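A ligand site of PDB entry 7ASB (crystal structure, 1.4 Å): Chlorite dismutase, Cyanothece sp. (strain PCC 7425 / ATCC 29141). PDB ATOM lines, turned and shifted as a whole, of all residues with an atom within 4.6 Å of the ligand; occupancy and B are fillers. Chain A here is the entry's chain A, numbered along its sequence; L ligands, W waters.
O1 of the ligand is in hydrogen-bond range of N of Ala 68 (2.9 Å). A ring nitrogen (NE2) of His 120 is bound to an iron atom (FE1) of the ligand (2.1 Å). O4 of the ligand is in salt-bridge range of NZ of Lys 98 (2.8 Å). The backbone NH (N) of Tyr 67 sits at hydrogen-bond distance from an oxygen (O1) of the ligand, at 2.8 Å. The backbone NH (N) of Arg 66 lies within hydrogen-bond range of an oxygen (O2) of the ligand (2.8 Å).
The backbone NH (N) of Phe 147 sits at hydrogen-bond distance from the backbone carbonyl oxygen (O) of Ile 96, at 3.0 Å. The side-chain hydroxyl (OG1) of Thr 149 lies within hydrogen-bond range of the backbone carbonyl oxygen (O) of Ile 94 (2.7 Å). OE2 of Glu 173 lies within salt-bridge range of NZ of Lys 98 (2.7 Å). The backbone carbonyl oxygen (O) of Phe 114 lies within hydrogen-bond range of the backbone NH (N) of His 120 (3.1 Å). NE1 of Trp 174 sits at hydrogen-bond distance from OE1 of Glu 180 (2.8 Å). The guanidinium group (NE) of Arg 66 lies within hydrogen-bond range of the backbone carbonyl oxygen (O) of Asn 64 (3.1 Å). The side-chain carboxylate (OE1) of Glu 173 sits at hydrogen-bond distance from a ring nitrogen (ND1) of His 120 (2.7 Å).
CG2 of Ile 65 touches O1 of the ligand, at 3.5 Å. Leu 76 touches the ligand (CD2 to C17, 3.7 Å). CD1 of Ile 94 touches C26 of the ligand, at 3.99 Å. Ile 96 touches the ligand. Trp 102 touches the ligand. Phe 114 touches the ligand (CZ to C6, 3.5 Å). OG1 of Thr 121 touches C9 of the ligand, 3.3 Å away. O of Gly 124 touches C18 of the ligand (3.3 Å). N of Leu 125 touches C17 of the ligand, at 3.96 Å. Leu 128 touches the ligand. Val 131 touches the ligand (CG1 to C19, 3.8 Å). Arg 133 touches the ligand. CD2 of Leu 135 touches C1 of the ligand, at 3.7 Å. Phe 147 touches the ligand. CG2 of Thr 149 touches C4 of the ligand, at 3.8 Å. Phe 151 touches the ligand (CZ to C21, 3.1 Å). Leu 164 touches the ligand (CD2 to C19, 3.6 Å). CD2 of Leu 165 touches C26 of the ligand, 3.7 Å away. SD of Met 168 touches C21 of the ligand, at 3.4 Å. Trp 174 touches the ligand (CZ2 to C26, 3.6 Å). Hydrophobic or aromatic side chains within 4 Å of the ligand: Ile 65, Tyr 67, Ala 68, Leu 76, Ile 94, Ile 96, Trp 102, Phe 114, His 120, Leu 128, Val 131, Leu 135, Phe 147, Phe 151, Leu 164, Leu 165, Met 168 and Trp 174.
Water W1 lies within hydrogen-bond range of an oxygen (O4) of the ligand, the side-chain hydroxyl (OH) of Tyr 67 and the indole nitrogen (NE1) of Trp 102. Water W3 lies within hydrogen-bond range of O2 of the ligand (2.8 Å) and O of Asn 64 (2.8 Å).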
ATOM      1  N   ASN A  64     -13.842 -23.115  14.201  1.00  0.00           N
ATOM      2  CA  ASN A  64     -13.278 -23.744  13.027  1.00  0.00           C
ATOM      3  C   ASN A  64     -14.090 -24.964  12.580  1.00  0.00           C
ATOM      4  O   ASN A  64     -14.861 -25.560  13.330  1.00  0.00           O
ATOM      5  CB  ASN A  64     -11.808 -24.122  13.259  1.00  0.00           C
ATOM      6  CG  ASN A  64     -11.658 -25.128  14.377  1.00  0.00           C
ATOM      7  OD1 ASN A  64     -11.748 -24.739  15.514  1.00  0.00           O
ATOM      8  ND2 ASN A  64     -11.539 -26.414  14.058  1.00  0.00           N
ATOM      9  N   ILE A  65     -13.872 -25.305  11.325  1.00  0.00           N
ATOM     10  CA  ILE A  65     -14.458 -26.467  10.683  1.00  0.00           C
ATOM     11  C   ILE A  65     -13.986 -27.726  11.375  1.00  0.00           C
ATOM     12  O   ILE A  65     -12.789 -27.870  11.705  1.00  0.00           O
ATOM     13  CB  ILE A  65     -14.124 -26.449   9.176  1.00  0.00           C
ATOM     14  CG1 ILE A  65     -14.946 -25.391   8.429  1.00  0.00           C
ATOM     15  CG2 ILE A  65     -14.223 -27.821   8.516  1.00  0.00           C
ATOM     16  CD1 ILE A  65     -16.411 -25.652   8.391  1.00  0.00           C
ATOM     17  N   ARG A  66     -14.905 -28.652  11.597  1.00  0.00           N
ATOM     18  CA  ARG A  66     -14.704 -29.909  12.307  1.00  0.00           C
ATOM     19  C   ARG A  66     -14.738 -31.155  11.428  1.00  0.00           C
ATOM     20  O   ARG A  66     -14.231 -32.192  11.819  1.00  0.00           O
ATOM     21  CB  ARG A  66     -15.698 -30.057  13.484  1.00  0.00           C
ATOM     22  CG  ARG A  66     -15.797 -28.844  14.384  1.00  0.00           C
ATOM     23  CD  ARG A  66     -14.413 -28.427  14.961  1.00  0.00           C
ATOM     24  NE  ARG A  66     -14.591 -27.306  15.839  1.00  0.00           N
ATOM     25  CZ  ARG A  66     -14.985 -27.363  17.088  1.00  0.00           C
ATOM     26  NH1 ARG A  66     -15.226 -28.554  17.657  1.00  0.00           N
ATOM     27  NH2 ARG A  66     -15.122 -26.274  17.813  1.00  0.00           N
ATOM     28  N   TYR A  67     -15.505 -31.110  10.277  1.00  0.00           N
ATOM     29  CA  TYR A  67     -15.801 -32.272   9.439  1.00  0.00           C
ATOM     30  C   TYR A  67     -15.617 -31.996   7.961  1.00  0.00           C
ATOM     31  O   TYR A  67     -15.111 -32.862   7.261  1.00  0.00           O
ATOM     32  CB  TYR A  67     -17.242 -32.788   9.708  1.00  0.00           C
ATOM     33  CG  TYR A  67     -17.415 -33.306  11.106  1.00  0.00           C
ATOM     34  CD1 TYR A  67     -16.754 -34.448  11.526  1.00  0.00           C
ATOM     35  CD2 TYR A  67     -18.212 -32.628  12.032  1.00  0.00           C
ATOM     36  CE1 TYR A  67     -16.872 -34.925  12.833  1.00  0.00           C
ATOM     37  CE2 TYR A  67     -18.332 -33.099  13.346  1.00  0.00           C
ATOM     38  CZ  TYR A  67     -17.650 -34.233  13.738  1.00  0.00           C
ATOM     39  OH  TYR A  67     -17.757 -34.740  14.992  1.00  0.00           O
ATOM     40  N   ALA A  68     -16.011 -30.822   7.477  1.00  0.00           N
ATOM     41  CA  ALA A  68     -16.017 -30.592   6.055  1.00  0.00           C
ATOM     42  C   ALA A  68     -14.600 -30.623   5.463  1.00  0.00           C
ATOM     43  O   ALA A  68     -13.640 -30.113   6.056  1.00  0.00           O
ATOM     44  CB  ALA A  68     -16.693 -29.255   5.730  1.00  0.00           C
ATOM     45  N   LEU A  76     -19.787 -25.576  -0.987  1.00  0.00           N
ATOM     46  CA  LEU A  76     -20.497 -24.631  -0.127  1.00  0.00           C
ATOM     47  C   LEU A  76     -20.234 -23.183  -0.522  1.00  0.00           C
ATOM     48  O   LEU A  76     -21.157 -22.378  -0.629  1.00  0.00           O
ATOM     49  CB  LEU A  76     -20.155 -24.851   1.338  1.00  0.00           C
ATOM     50  CG  LEU A  76     -20.693 -26.162   1.864  1.00  0.00           C
ATOM     51  CD1 LEU A  76     -19.902 -26.608   3.095  1.00  0.00           C
ATOM     52  CD2 LEU A  76     -22.186 -26.083   2.241  1.00  0.00           C
ATOM     53  N   ILE A  94     -32.358 -23.544  16.064  1.00  0.00           N
ATOM     54  CA  ILE A  94     -32.558 -24.945  16.435  1.00  0.00           C
ATOM     55  C   ILE A  94     -31.417 -25.395  17.342  1.00  0.00           C
ATOM     56  O   ILE A  94     -30.350 -25.792  16.830  1.00  0.00           O
ATOM     57  CB  ILE A  94     -32.693 -25.875  15.213  1.00  0.00           C
ATOM     58  CG1 ILE A  94     -33.833 -25.361  14.291  1.00  0.00           C
ATOM     59  CG2 ILE A  94     -32.992 -27.324  15.696  1.00  0.00           C
ATOM     60  CD1 ILE A  94     -33.914 -26.123  12.987  1.00  0.00           C
ATOM     61  N   ILE A  96     -29.451 -28.013  19.546  1.00  0.00           N
ATOM     62  CA  ILE A  96     -29.315 -29.455  19.401  1.00  0.00           C
ATOM     63  C   ILE A  96     -28.347 -29.953  20.454  1.00  0.00           C
ATOM     64  O   ILE A  96     -27.288 -29.358  20.695  1.00  0.00           O
ATOM     65  CB  ILE A  96     -28.798 -29.816  18.000  1.00  0.00           C
ATOM     66  CG1 ILE A  96     -29.921 -29.452  17.010  1.00  0.00           C
ATOM     67  CG2 ILE A  96     -28.356 -31.205  17.879  1.00  0.00           C
ATOM     68  CD1 ILE A  96     -29.474 -29.400  15.643  1.00  0.00           C
ATOM     69  N   LYS A  98     -26.297 -33.679  21.301  1.00  0.00           N
ATOM     70  CA  LYS A  98     -25.993 -35.049  20.904  1.00  0.00           C
ATOM     71  C   LYS A  98     -25.586 -35.875  22.123  1.00  0.00           C
ATOM     72  O   LYS A  98     -25.261 -35.334  23.172  1.00  0.00           O
ATOM     73  CB  LYS A  98     -24.882 -35.070  19.858  1.00  0.00           C
ATOM     74  CG  LYS A  98     -25.296 -34.429  18.528  1.00  0.00           C
ATOM     75  CD  LYS A  98     -24.230 -34.646  17.440  1.00  0.00           C
ATOM     76  CE  LYS A  98     -24.757 -34.144  16.108  1.00  0.00           C
ATOM     77  NZ  LYS A  98     -23.773 -34.474  14.989  1.00  0.00           N
ATOM     78  N   TRP A 102     -22.121 -40.332  21.096  1.00  0.00           N
ATOM     79  CA  TRP A 102     -21.554 -39.595  19.983  1.00  0.00           C
ATOM     80  C   TRP A 102     -20.208 -39.018  20.362  1.00  0.00           C
ATOM     81  O   TRP A 102     -19.207 -39.157  19.626  1.00  0.00           O
ATOM     82  CB  TRP A 102     -22.503 -38.471  19.595  1.00  0.00           C
ATOM     83  CG  TRP A 102     -21.941 -37.489  18.575  1.00  0.00           C
ATOM     84  CD1 TRP A 102     -21.381 -36.287  18.830  1.00  0.00           C
ATOM     85  CD2 TRP A 102     -21.826 -37.728  17.198  1.00  0.00           C
ATOM     86  NE1 TRP A 102     -20.963 -35.701  17.647  1.00  0.00           N
ATOM     87  CE2 TRP A 102     -21.226 -36.576  16.629  1.00  0.00           C
ATOM     88  CE3 TRP A 102     -22.238 -38.788  16.333  1.00  0.00           C
ATOM     89  CZ2 TRP A 102     -20.978 -36.446  15.244  1.00  0.00           C
ATOM     90  CZ3 TRP A 102     -21.988 -38.681  14.985  1.00  0.00           C
ATOM     91  CH2 TRP A 102     -21.366 -37.504  14.439  1.00  0.00           C
ATOM     92  N   PHE A 114     -21.390 -38.641   9.911  1.00  0.00           N
ATOM     93  CA  PHE A 114     -21.848 -37.304   9.495  1.00  0.00           C
ATOM     94  C   PHE A 114     -22.022 -37.202   7.990  1.00  0.00           C
ATOM     95  O   PHE A 114     -23.083 -36.782   7.492  1.00  0.00           O
ATOM     96  CB  PHE A 114     -20.829 -36.269   9.989  1.00  0.00           C
ATOM     97  CG  PHE A 114     -21.134 -34.847   9.595  1.00  0.00           C
ATOM     98  CD1 PHE A 114     -22.026 -34.052  10.319  1.00  0.00           C
ATOM     99  CD2 PHE A 114     -20.525 -34.287   8.475  1.00  0.00           C
ATOM    100  CE1 PHE A 114     -22.272 -32.771   9.973  1.00  0.00           C
ATOM    101  CE2 PHE A 114     -20.798 -32.979   8.110  1.00  0.00           C
ATOM    102  CZ  PHE A 114     -21.649 -32.208   8.853  1.00  0.00           C
ATOM    103  N   HIS A 120     -24.791 -35.352   5.360  1.00  0.00           N
ATOM    104  CA  HIS A 120     -25.238 -34.070   5.907  1.00  0.00           C
ATOM    105  C   HIS A 120     -24.995 -32.893   4.952  1.00  0.00           C
ATOM    106  O   HIS A 120     -25.922 -32.115   4.662  1.00  0.00           O
ATOM    107  CB  HIS A 120     -24.562 -33.843   7.255  1.00  0.00           C
ATOM    108  CG  HIS A 120     -25.056 -32.638   8.010  1.00  0.00           C
ATOM    109  ND1 HIS A 120     -25.572 -32.708   9.278  1.00  0.00           N
ATOM    110  CD2 HIS A 120     -25.104 -31.332   7.655  1.00  0.00           C
ATOM    111  CE1 HIS A 120     -25.852 -31.479   9.699  1.00  0.00           C
ATOM    112  NE2 HIS A 120     -25.620 -30.625   8.716  1.00  0.00           N
ATOM    113  N   THR A 121     -23.754 -32.712   4.489  1.00  0.00           N
ATOM    114  CA  THR A 121     -23.444 -31.589   3.589  1.00  0.00           C
ATOM    115  C   THR A 121     -24.101 -31.762   2.211  1.00  0.00           C
ATOM    116  O   THR A 121     -24.583 -30.776   1.638  1.00  0.00           O
ATOM    117  CB  THR A 121     -21.931 -31.463   3.486  1.00  0.00           C
ATOM    118  OG1 THR A 121     -21.353 -31.271   4.784  1.00  0.00           O
ATOM    119  CG2 THR A 121     -21.565 -30.281   2.617  1.00  0.00           C
ATOM    120  N   GLY A 124     -27.723 -30.908   2.652  1.00  0.00           N
ATOM    121  CA  GLY A 124     -27.925 -29.504   2.923  1.00  0.00           C
ATOM    122  C   GLY A 124     -27.708 -28.640   1.706  1.00  0.00           C
ATOM    123  O   GLY A 124     -28.408 -27.637   1.498  1.00  0.00           O
ATOM    124  N   LEU A 125     -26.713 -29.004   0.869  1.00  0.00           N
ATOM    125  CA  LEU A 125     -26.430 -28.210  -0.321  1.00  0.00           C
ATOM    126  C   LEU A 125     -27.615 -28.126  -1.253  1.00  0.00           C
ATOM    127  O   LEU A 125     -27.703 -27.173  -2.044  1.00  0.00           O
ATOM    128  CB  LEU A 125     -25.293 -28.853  -1.114  1.00  0.00           C
ATOM    129  CG  LEU A 125     -23.864 -28.430  -0.695  1.00  0.00           C
ATOM    130  CD1 LEU A 125     -22.812 -29.377  -1.224  1.00  0.00           C
ATOM    131  CD2 LEU A 125     -23.606 -27.044  -1.215  1.00  0.00           C
ATOM    132  N   LEU A 128     -29.499 -24.826  -0.759  1.00  0.00           N
ATOM    133  CA  LEU A 128     -28.872 -23.562  -1.051  1.00  0.00           C
ATOM    134  C   LEU A 128     -29.093 -23.234  -2.526  1.00  0.00           C
ATOM    135  O   LEU A 128     -29.133 -24.153  -3.372  1.00  0.00           O
ATOM    136  CB  LEU A 128     -27.355 -23.655  -0.775  1.00  0.00           C
ATOM    137  CG  LEU A 128     -26.969 -23.505   0.699  1.00  0.00           C
ATOM    138  CD1 LEU A 128     -27.811 -24.278   1.699  1.00  0.00           C
ATOM    139  CD2 LEU A 128     -25.468 -23.816   0.893  1.00  0.00           C
ATOM    140  N   VAL A 131     -31.512 -21.132   1.628  1.00  0.00           N
ATOM    141  CA  VAL A 131     -31.328 -21.106   3.089  1.00  0.00           C
ATOM    142  C   VAL A 131     -29.916 -20.646   3.428  1.00  0.00           C
ATOM    143  O   VAL A 131     -28.942 -21.256   2.986  1.00  0.00           O
ATOM    144  CB  VAL A 131     -31.583 -22.491   3.663  1.00  0.00           C
ATOM    145  CG1 VAL A 131     -31.433 -22.459   5.179  1.00  0.00           C
ATOM    146  CG2 VAL A 131     -33.040 -22.918   3.337  1.00  0.00           C
ATOM    147  N   ARG A 133     -27.268 -19.819   6.743  1.00  0.00           N
ATOM    148  CA  ARG A 133     -27.097 -20.554   8.007  1.00  0.00           C
ATOM    149  C   ARG A 133     -25.897 -20.036   8.785  1.00  0.00           C
ATOM    150  O   ARG A 133     -24.992 -19.421   8.249  1.00  0.00           O
ATOM    151  CB  ARG A 133     -26.996 -22.054   7.726  1.00  0.00           C
ATOM    152  CG  ARG A 133     -25.622 -22.476   7.185  1.00  0.00           C
ATOM    153  CD  ARG A 133     -25.537 -23.888   6.626  1.00  0.00           C
ATOM    154  NE  ARG A 133     -24.129 -24.233   6.480  1.00  0.00           N
ATOM    155  CZ  ARG A 133     -23.358 -23.862   5.453  1.00  0.00           C
ATOM    156  NH1 ARG A 133     -23.864 -23.175   4.455  1.00  0.00           N
ATOM    157  NH2 ARG A 133     -22.050 -24.109   5.479  1.00  0.00           N
ATOM    158  N   LEU A 135     -23.582 -21.783  12.255  1.00  0.00           N
ATOM    159  CA  LEU A 135     -23.382 -22.833  13.234  1.00  0.00           C
ATOM    160  C   LEU A 135     -22.607 -22.268  14.414  1.00  0.00           C
ATOM    161  O   LEU A 135     -21.524 -21.680  14.242  1.00  0.00           O
ATOM    162  CB  LEU A 135     -22.613 -23.972  12.594  1.00  0.00           C
ATOM    163  CG  LEU A 135     -22.134 -25.108  13.507  1.00  0.00           C
ATOM    164  CD1 LEU A 135     -23.373 -25.815  14.129  1.00  0.00           C
ATOM    165  CD2 LEU A 135     -21.320 -26.088  12.736  1.00  0.00           C
ATOM    166  N   PHE A 147     -25.079 -27.428  20.329  1.00  0.00           N
ATOM    167  CA  PHE A 147     -24.975 -26.537  19.180  1.00  0.00           C
ATOM    168  C   PHE A 147     -26.148 -25.598  19.186  1.00  0.00           C
ATOM    169  O   PHE A 147     -27.254 -25.954  19.637  1.00  0.00           O
ATOM    170  CB  PHE A 147     -25.015 -27.302  17.836  1.00  0.00           C
ATOM    171  CG  PHE A 147     -24.009 -28.412  17.773  1.00  0.00           C
ATOM    172  CD1 PHE A 147     -22.688 -28.107  17.427  1.00  0.00           C
ATOM    173  CD2 PHE A 147     -24.318 -29.721  18.044  1.00  0.00           C
ATOM    174  CE1 PHE A 147     -21.708 -29.054  17.416  1.00  0.00           C
ATOM    175  CE2 PHE A 147     -23.379 -30.694  17.962  1.00  0.00           C
ATOM    176  CZ  PHE A 147     -22.043 -30.372  17.661  1.00  0.00           C
ATOM    177  N   THR A 149     -27.972 -23.837  16.047  1.00  0.00           N
ATOM    178  CA  THR A 149     -27.993 -23.757  14.605  1.00  0.00           C
ATOM    179  C   THR A 149     -28.967 -22.669  14.174  1.00  0.00           C
ATOM    180  O   THR A 149     -30.061 -22.550  14.750  1.00  0.00           O
ATOM    181  CB  THR A 149     -28.240 -25.111  13.929  1.00  0.00           C
ATOM    182  OG1 THR A 149     -29.569 -25.552  14.216  1.00  0.00           O
ATOM    183  CG2 THR A 149     -27.229 -26.124  14.412  1.00  0.00           C
ATOM    184  N   PHE A 151     -30.875 -20.611  10.825  1.00  0.00           N
ATOM    185  CA  PHE A 151     -31.262 -20.655   9.421  1.00  0.00           C
ATOM    186  C   PHE A 151     -32.165 -19.473   9.117  1.00  0.00           C
ATOM    187  O   PHE A 151     -32.986 -19.081   9.964  1.00  0.00           O
ATOM    188  CB  PHE A 151     -32.000 -22.004   9.084  1.00  0.00           C
ATOM    189  CG  PHE A 151     -31.156 -23.158   9.511  1.00  0.00           C
ATOM    190  CD1 PHE A 151     -30.156 -23.639   8.684  1.00  0.00           C
ATOM    191  CD2 PHE A 151     -31.358 -23.757  10.767  1.00  0.00           C
ATOM    192  CE1 PHE A 151     -29.333 -24.646   9.124  1.00  0.00           C
ATOM    193  CE2 PHE A 151     -30.519 -24.740  11.217  1.00  0.00           C
ATOM    194  CZ  PHE A 151     -29.493 -25.205  10.383  1.00  0.00           C
ATOM    195  N   PHE A 161     -37.521 -25.851   3.546  1.00  0.00           N
ATOM    196  CA  PHE A 161     -36.821 -25.983   4.813  1.00  0.00           C
ATOM    197  C   PHE A 161     -37.473 -27.062   5.674  1.00  0.00           C
ATOM    198  O   PHE A 161     -36.792 -27.884   6.292  1.00  0.00           O
ATOM    199  CB  PHE A 161     -36.777 -24.652   5.563  1.00  0.00           C
ATOM    200  CG  PHE A 161     -35.901 -24.711   6.772  1.00  0.00           C
ATOM    201  CD1 PHE A 161     -34.501 -24.757   6.684  1.00  0.00           C
ATOM    202  CD2 PHE A 161     -36.460 -24.814   8.044  1.00  0.00           C
ATOM    203  CE1 PHE A 161     -33.717 -24.872   7.820  1.00  0.00           C
ATOM    204  CE2 PHE A 161     -35.685 -24.911   9.148  1.00  0.00           C
ATOM    205  CZ  PHE A 161     -34.292 -24.924   9.055  1.00  0.00           C
ATOM    206  N   LEU A 164     -36.269 -30.386   4.460  1.00  0.00           N
ATOM    207  CA  LEU A 164     -34.904 -30.600   4.913  1.00  0.00           C
ATOM    208  C   LEU A 164     -34.906 -31.106   6.335  1.00  0.00           C
ATOM    209  O   LEU A 164     -34.237 -32.100   6.650  1.00  0.00           O
ATOM    210  CB  LEU A 164     -34.121 -29.284   4.825  1.00  0.00           C
ATOM    211  CG  LEU A 164     -32.727 -29.342   5.489  1.00  0.00           C
ATOM    212  CD1 LEU A 164     -31.949 -30.421   4.838  1.00  0.00           C
ATOM    213  CD2 LEU A 164     -32.144 -27.984   5.306  1.00  0.00           C
ATOM    214  N   LEU A 165     -35.688 -30.484   7.219  1.00  0.00           N
ATOM    215  CA  LEU A 165     -35.721 -30.943   8.603  1.00  0.00           C
ATOM    216  C   LEU A 165     -36.104 -32.409   8.691  1.00  0.00           C
ATOM    217  O   LEU A 165     -35.524 -33.185   9.446  1.00  0.00           O
ATOM    218  CB  LEU A 165     -36.655 -30.096   9.461  1.00  0.00           C
ATOM    219  CG  LEU A 165     -36.334 -28.612   9.683  1.00  0.00           C
ATOM    220  CD1 LEU A 165     -37.430 -27.990  10.478  1.00  0.00           C
ATOM    221  CD2 LEU A 165     -34.988 -28.592  10.469  1.00  0.00           C
ATOM    222  N   MET A 168     -33.212 -34.663   7.548  1.00  0.00           N
ATOM    223  CA  MET A 168     -32.118 -34.800   8.503  1.00  0.00           C
ATOM    224  C   MET A 168     -32.535 -35.669   9.668  1.00  0.00           C
ATOM    225  O   MET A 168     -31.732 -36.480  10.172  1.00  0.00           O
ATOM    226  CB  MET A 168     -31.724 -33.423   8.980  1.00  0.00           C
ATOM    227  CG  MET A 168     -31.249 -32.641   7.787  1.00  0.00           C
ATOM    228  SD  MET A 168     -30.397 -31.142   8.075  1.00  0.00           S
ATOM    229  CE  MET A 168     -29.030 -31.867   8.963  1.00  0.00           C
ATOM    230  N   GLU A 173     -27.066 -39.846  11.650  1.00  0.00           N
ATOM    231  CA  GLU A 173     -26.558 -38.831  12.555  1.00  0.00           C
ATOM    232  C   GLU A 173     -27.578 -38.471  13.650  1.00  0.00           C
ATOM    233  O   GLU A 173     -27.239 -38.339  14.824  1.00  0.00           O
ATOM    234  CB  GLU A 173     -26.162 -37.588  11.776  1.00  0.00           C
ATOM    235  CG  GLU A 173     -25.723 -36.448  12.618  1.00  0.00           C
ATOM    236  CD  GLU A 173     -25.389 -35.191  11.864  1.00  0.00           C
ATOM    237  OE1 GLU A 173     -25.724 -35.083  10.653  1.00  0.00           O
ATOM    238  OE2 GLU A 173     -24.811 -34.242  12.491  1.00  0.00           O
ATOM    239  N   TRP A 174     -28.849 -38.261  13.227  1.00  0.00           N
ATOM    240  CA  TRP A 174     -29.963 -38.067  14.144  1.00  0.00           C
ATOM    241  C   TRP A 174     -30.268 -39.118  15.160  1.00  0.00           C
ATOM    242  O   TRP A 174     -30.878 -38.769  16.161  1.00  0.00           O
ATOM    243  CB  TRP A 174     -31.226 -37.381  13.568  1.00  0.00           C
ATOM    244  CG  TRP A 174     -31.392 -35.994  13.588  1.00  0.00           C
ATOM    245  CD1 TRP A 174     -32.208 -35.369  14.543  1.00  0.00           C
ATOM    246  CD2 TRP A 174     -30.578 -34.938  13.097  1.00  0.00           C
ATOM    247  NE1 TRP A 174     -32.128 -34.042  14.467  1.00  0.00           N
ATOM    248  CE2 TRP A 174     -31.064 -33.720  13.677  1.00  0.00           C
ATOM    249  CE3 TRP A 174     -29.485 -34.873  12.229  1.00  0.00           C
ATOM    250  CZ2 TRP A 174     -30.561 -32.499  13.333  1.00  0.00           C
ATOM    251  CZ3 TRP A 174     -28.987 -33.608  11.900  1.00  0.00           C
ATOM    252  CH2 TRP A 174     -29.504 -32.439  12.475  1.00  0.00           C
ATOM    253  N   GLU A 180     -33.693 -31.448  21.034  1.00  0.00           N
ATOM    254  CA  GLU A 180     -33.832 -30.598  19.854  1.00  0.00           C
ATOM    255  C   GLU A 180     -35.092 -29.748  20.039  1.00  0.00           C
ATOM    256  O   GLU A 180     -36.157 -30.263  20.440  1.00  0.00           O
ATOM    257  CB  GLU A 180     -33.921 -31.450  18.561  1.00  0.00           C
ATOM    258  CG  GLU A 180     -34.075 -30.648  17.241  1.00  0.00           C
ATOM    259  CD  GLU A 180     -34.053 -31.510  15.948  1.00  0.00           C
ATOM    260  OE1 GLU A 180     -34.042 -32.750  16.080  1.00  0.00           O
ATOM    261  OE2 GLU A 180     -34.056 -30.946  14.816  1.00  0.00           O
HETATM  262  C1  LIG L   1     -22.804 -28.938  10.902  1.00  0.00           C
HETATM  263  C2  LIG L   1     -24.048 -27.798   6.326  1.00  0.00           C
HETATM  264  C3  LIG L   1     -28.755 -27.642   7.547  1.00  0.00           C
HETATM  265  C4  LIG L   1     -27.463 -29.058  12.042  1.00  0.00           C
HETATM  266  C5  LIG L   1     -22.674 -28.664   9.575  1.00  0.00           C
HETATM  267  C6  LIG L   1     -21.528 -28.696   8.700  1.00  0.00           C
HETATM  268  C7  LIG L   1     -21.858 -28.320   7.468  1.00  0.00           C
HETATM  269  C8  LIG L   1     -23.283 -28.139   7.455  1.00  0.00           C
HETATM  270  C9  LIG L   1     -20.968 -28.266   6.210  1.00  0.00           C
HETATM  271  C10 LIG L   1     -20.102 -29.058   9.194  1.00  0.00           C
HETATM  272  C11 LIG L   1     -19.325 -27.858   9.677  1.00  0.00           C
HETATM  273  C12 LIG L   1     -17.961 -28.363  10.187  1.00  0.00           C
HETATM  274  O1  LIG L   1     -17.297 -29.180   9.459  1.00  0.00           O
HETATM  275  O2  LIG L   1     -17.584 -27.978  11.321  1.00  0.00           O
HETATM  276  C13 LIG L   1     -25.431 -27.664   6.298  1.00  0.00           C
HETATM  277  C14 LIG L   1     -26.093 -27.084   5.174  1.00  0.00           C
HETATM  278  C15 LIG L   1     -27.389 -27.023   5.498  1.00  0.00           C
HETATM  279  C16 LIG L   1     -27.588 -27.503   6.827  1.00  0.00           C
HETATM  280  C17 LIG L   1     -25.452 -26.687   3.825  1.00  0.00           C
HETATM  281  C18 LIG L   1     -28.476 -26.460   4.587  1.00  0.00           C
HETATM  282  C19 LIG L   1     -29.393 -25.676   5.190  1.00  0.00           C
HETATM  283  C20 LIG L   1     -28.907 -28.088   8.831  1.00  0.00           C
HETATM  284  C21 LIG L   1     -30.044 -28.213   9.685  1.00  0.00           C
HETATM  285  C22 LIG L   1     -29.694 -28.575  10.896  1.00  0.00           C
HETATM  286  C23 LIG L   1     -28.236 -28.713  10.907  1.00  0.00           C
HETATM  287  C24 LIG L   1     -31.434 -27.950   9.111  1.00  0.00           C
HETATM  288  C25 LIG L   1     -30.524 -28.812  12.116  1.00  0.00           C
HETATM  289  C26 LIG L   1     -31.711 -29.308  12.011  1.00  0.00           C
HETATM  290  C27 LIG L   1     -26.070 -29.100  12.155  1.00  0.00           C
HETATM  291  C28 LIG L   1     -25.318 -29.495  13.343  1.00  0.00           C
HETATM  292  C29 LIG L   1     -24.041 -29.446  13.025  1.00  0.00           C
HETATM  293  C30 LIG L   1     -23.907 -29.052  11.659  1.00  0.00           C
HETATM  294  C31 LIG L   1     -25.961 -29.821  14.684  1.00  0.00           C
HETATM  295  C32 LIG L   1     -22.875 -29.730  13.967  1.00  0.00           C
HETATM  296  C33 LIG L   1     -22.474 -31.179  13.696  1.00  0.00           C
HETATM  297  C34 LIG L   1     -21.426 -31.675  14.633  1.00  0.00           C
HETATM  298  O3  LIG L   1     -20.380 -30.945  14.720  1.00  0.00           O
HETATM  299  O4  LIG L   1     -21.563 -32.791  15.231  1.00  0.00           O
HETATM  300  N1  LIG L   1     -23.839 -28.322   8.745  1.00  0.00           N
HETATM  301  N2  LIG L   1     -26.330 -27.860   7.324  1.00  0.00           N
HETATM  302  N3  LIG L   1     -27.714 -28.413   9.612  1.00  0.00           N
HETATM  303  N4  LIG L   1     -25.183 -28.827  11.138  1.00  0.00           N
HETATM  304 FE1  LIG L   1     -25.786 -28.550   9.148  1.00  0.00          FE
HETATM  305  O   HOH W   1     -19.456 -33.506  16.650  1.00  0.00           O
HETATM  306  O   HOH W   2     -18.264 -30.966  16.712  1.00  0.00           O
HETATM  307  O   HOH W   3     -17.619 -25.606  12.734  1.00  0.00           O
HETATM  308  O   HOH W   4     -23.121 -25.241   8.984  1.00  0.00           O
HETATM  309  O   HOH W   5     -19.201 -28.860  13.676  1.00  0.00           O
HETATM  310  O   HOH W   6     -25.356 -26.060   9.964  1.00  0.00           O
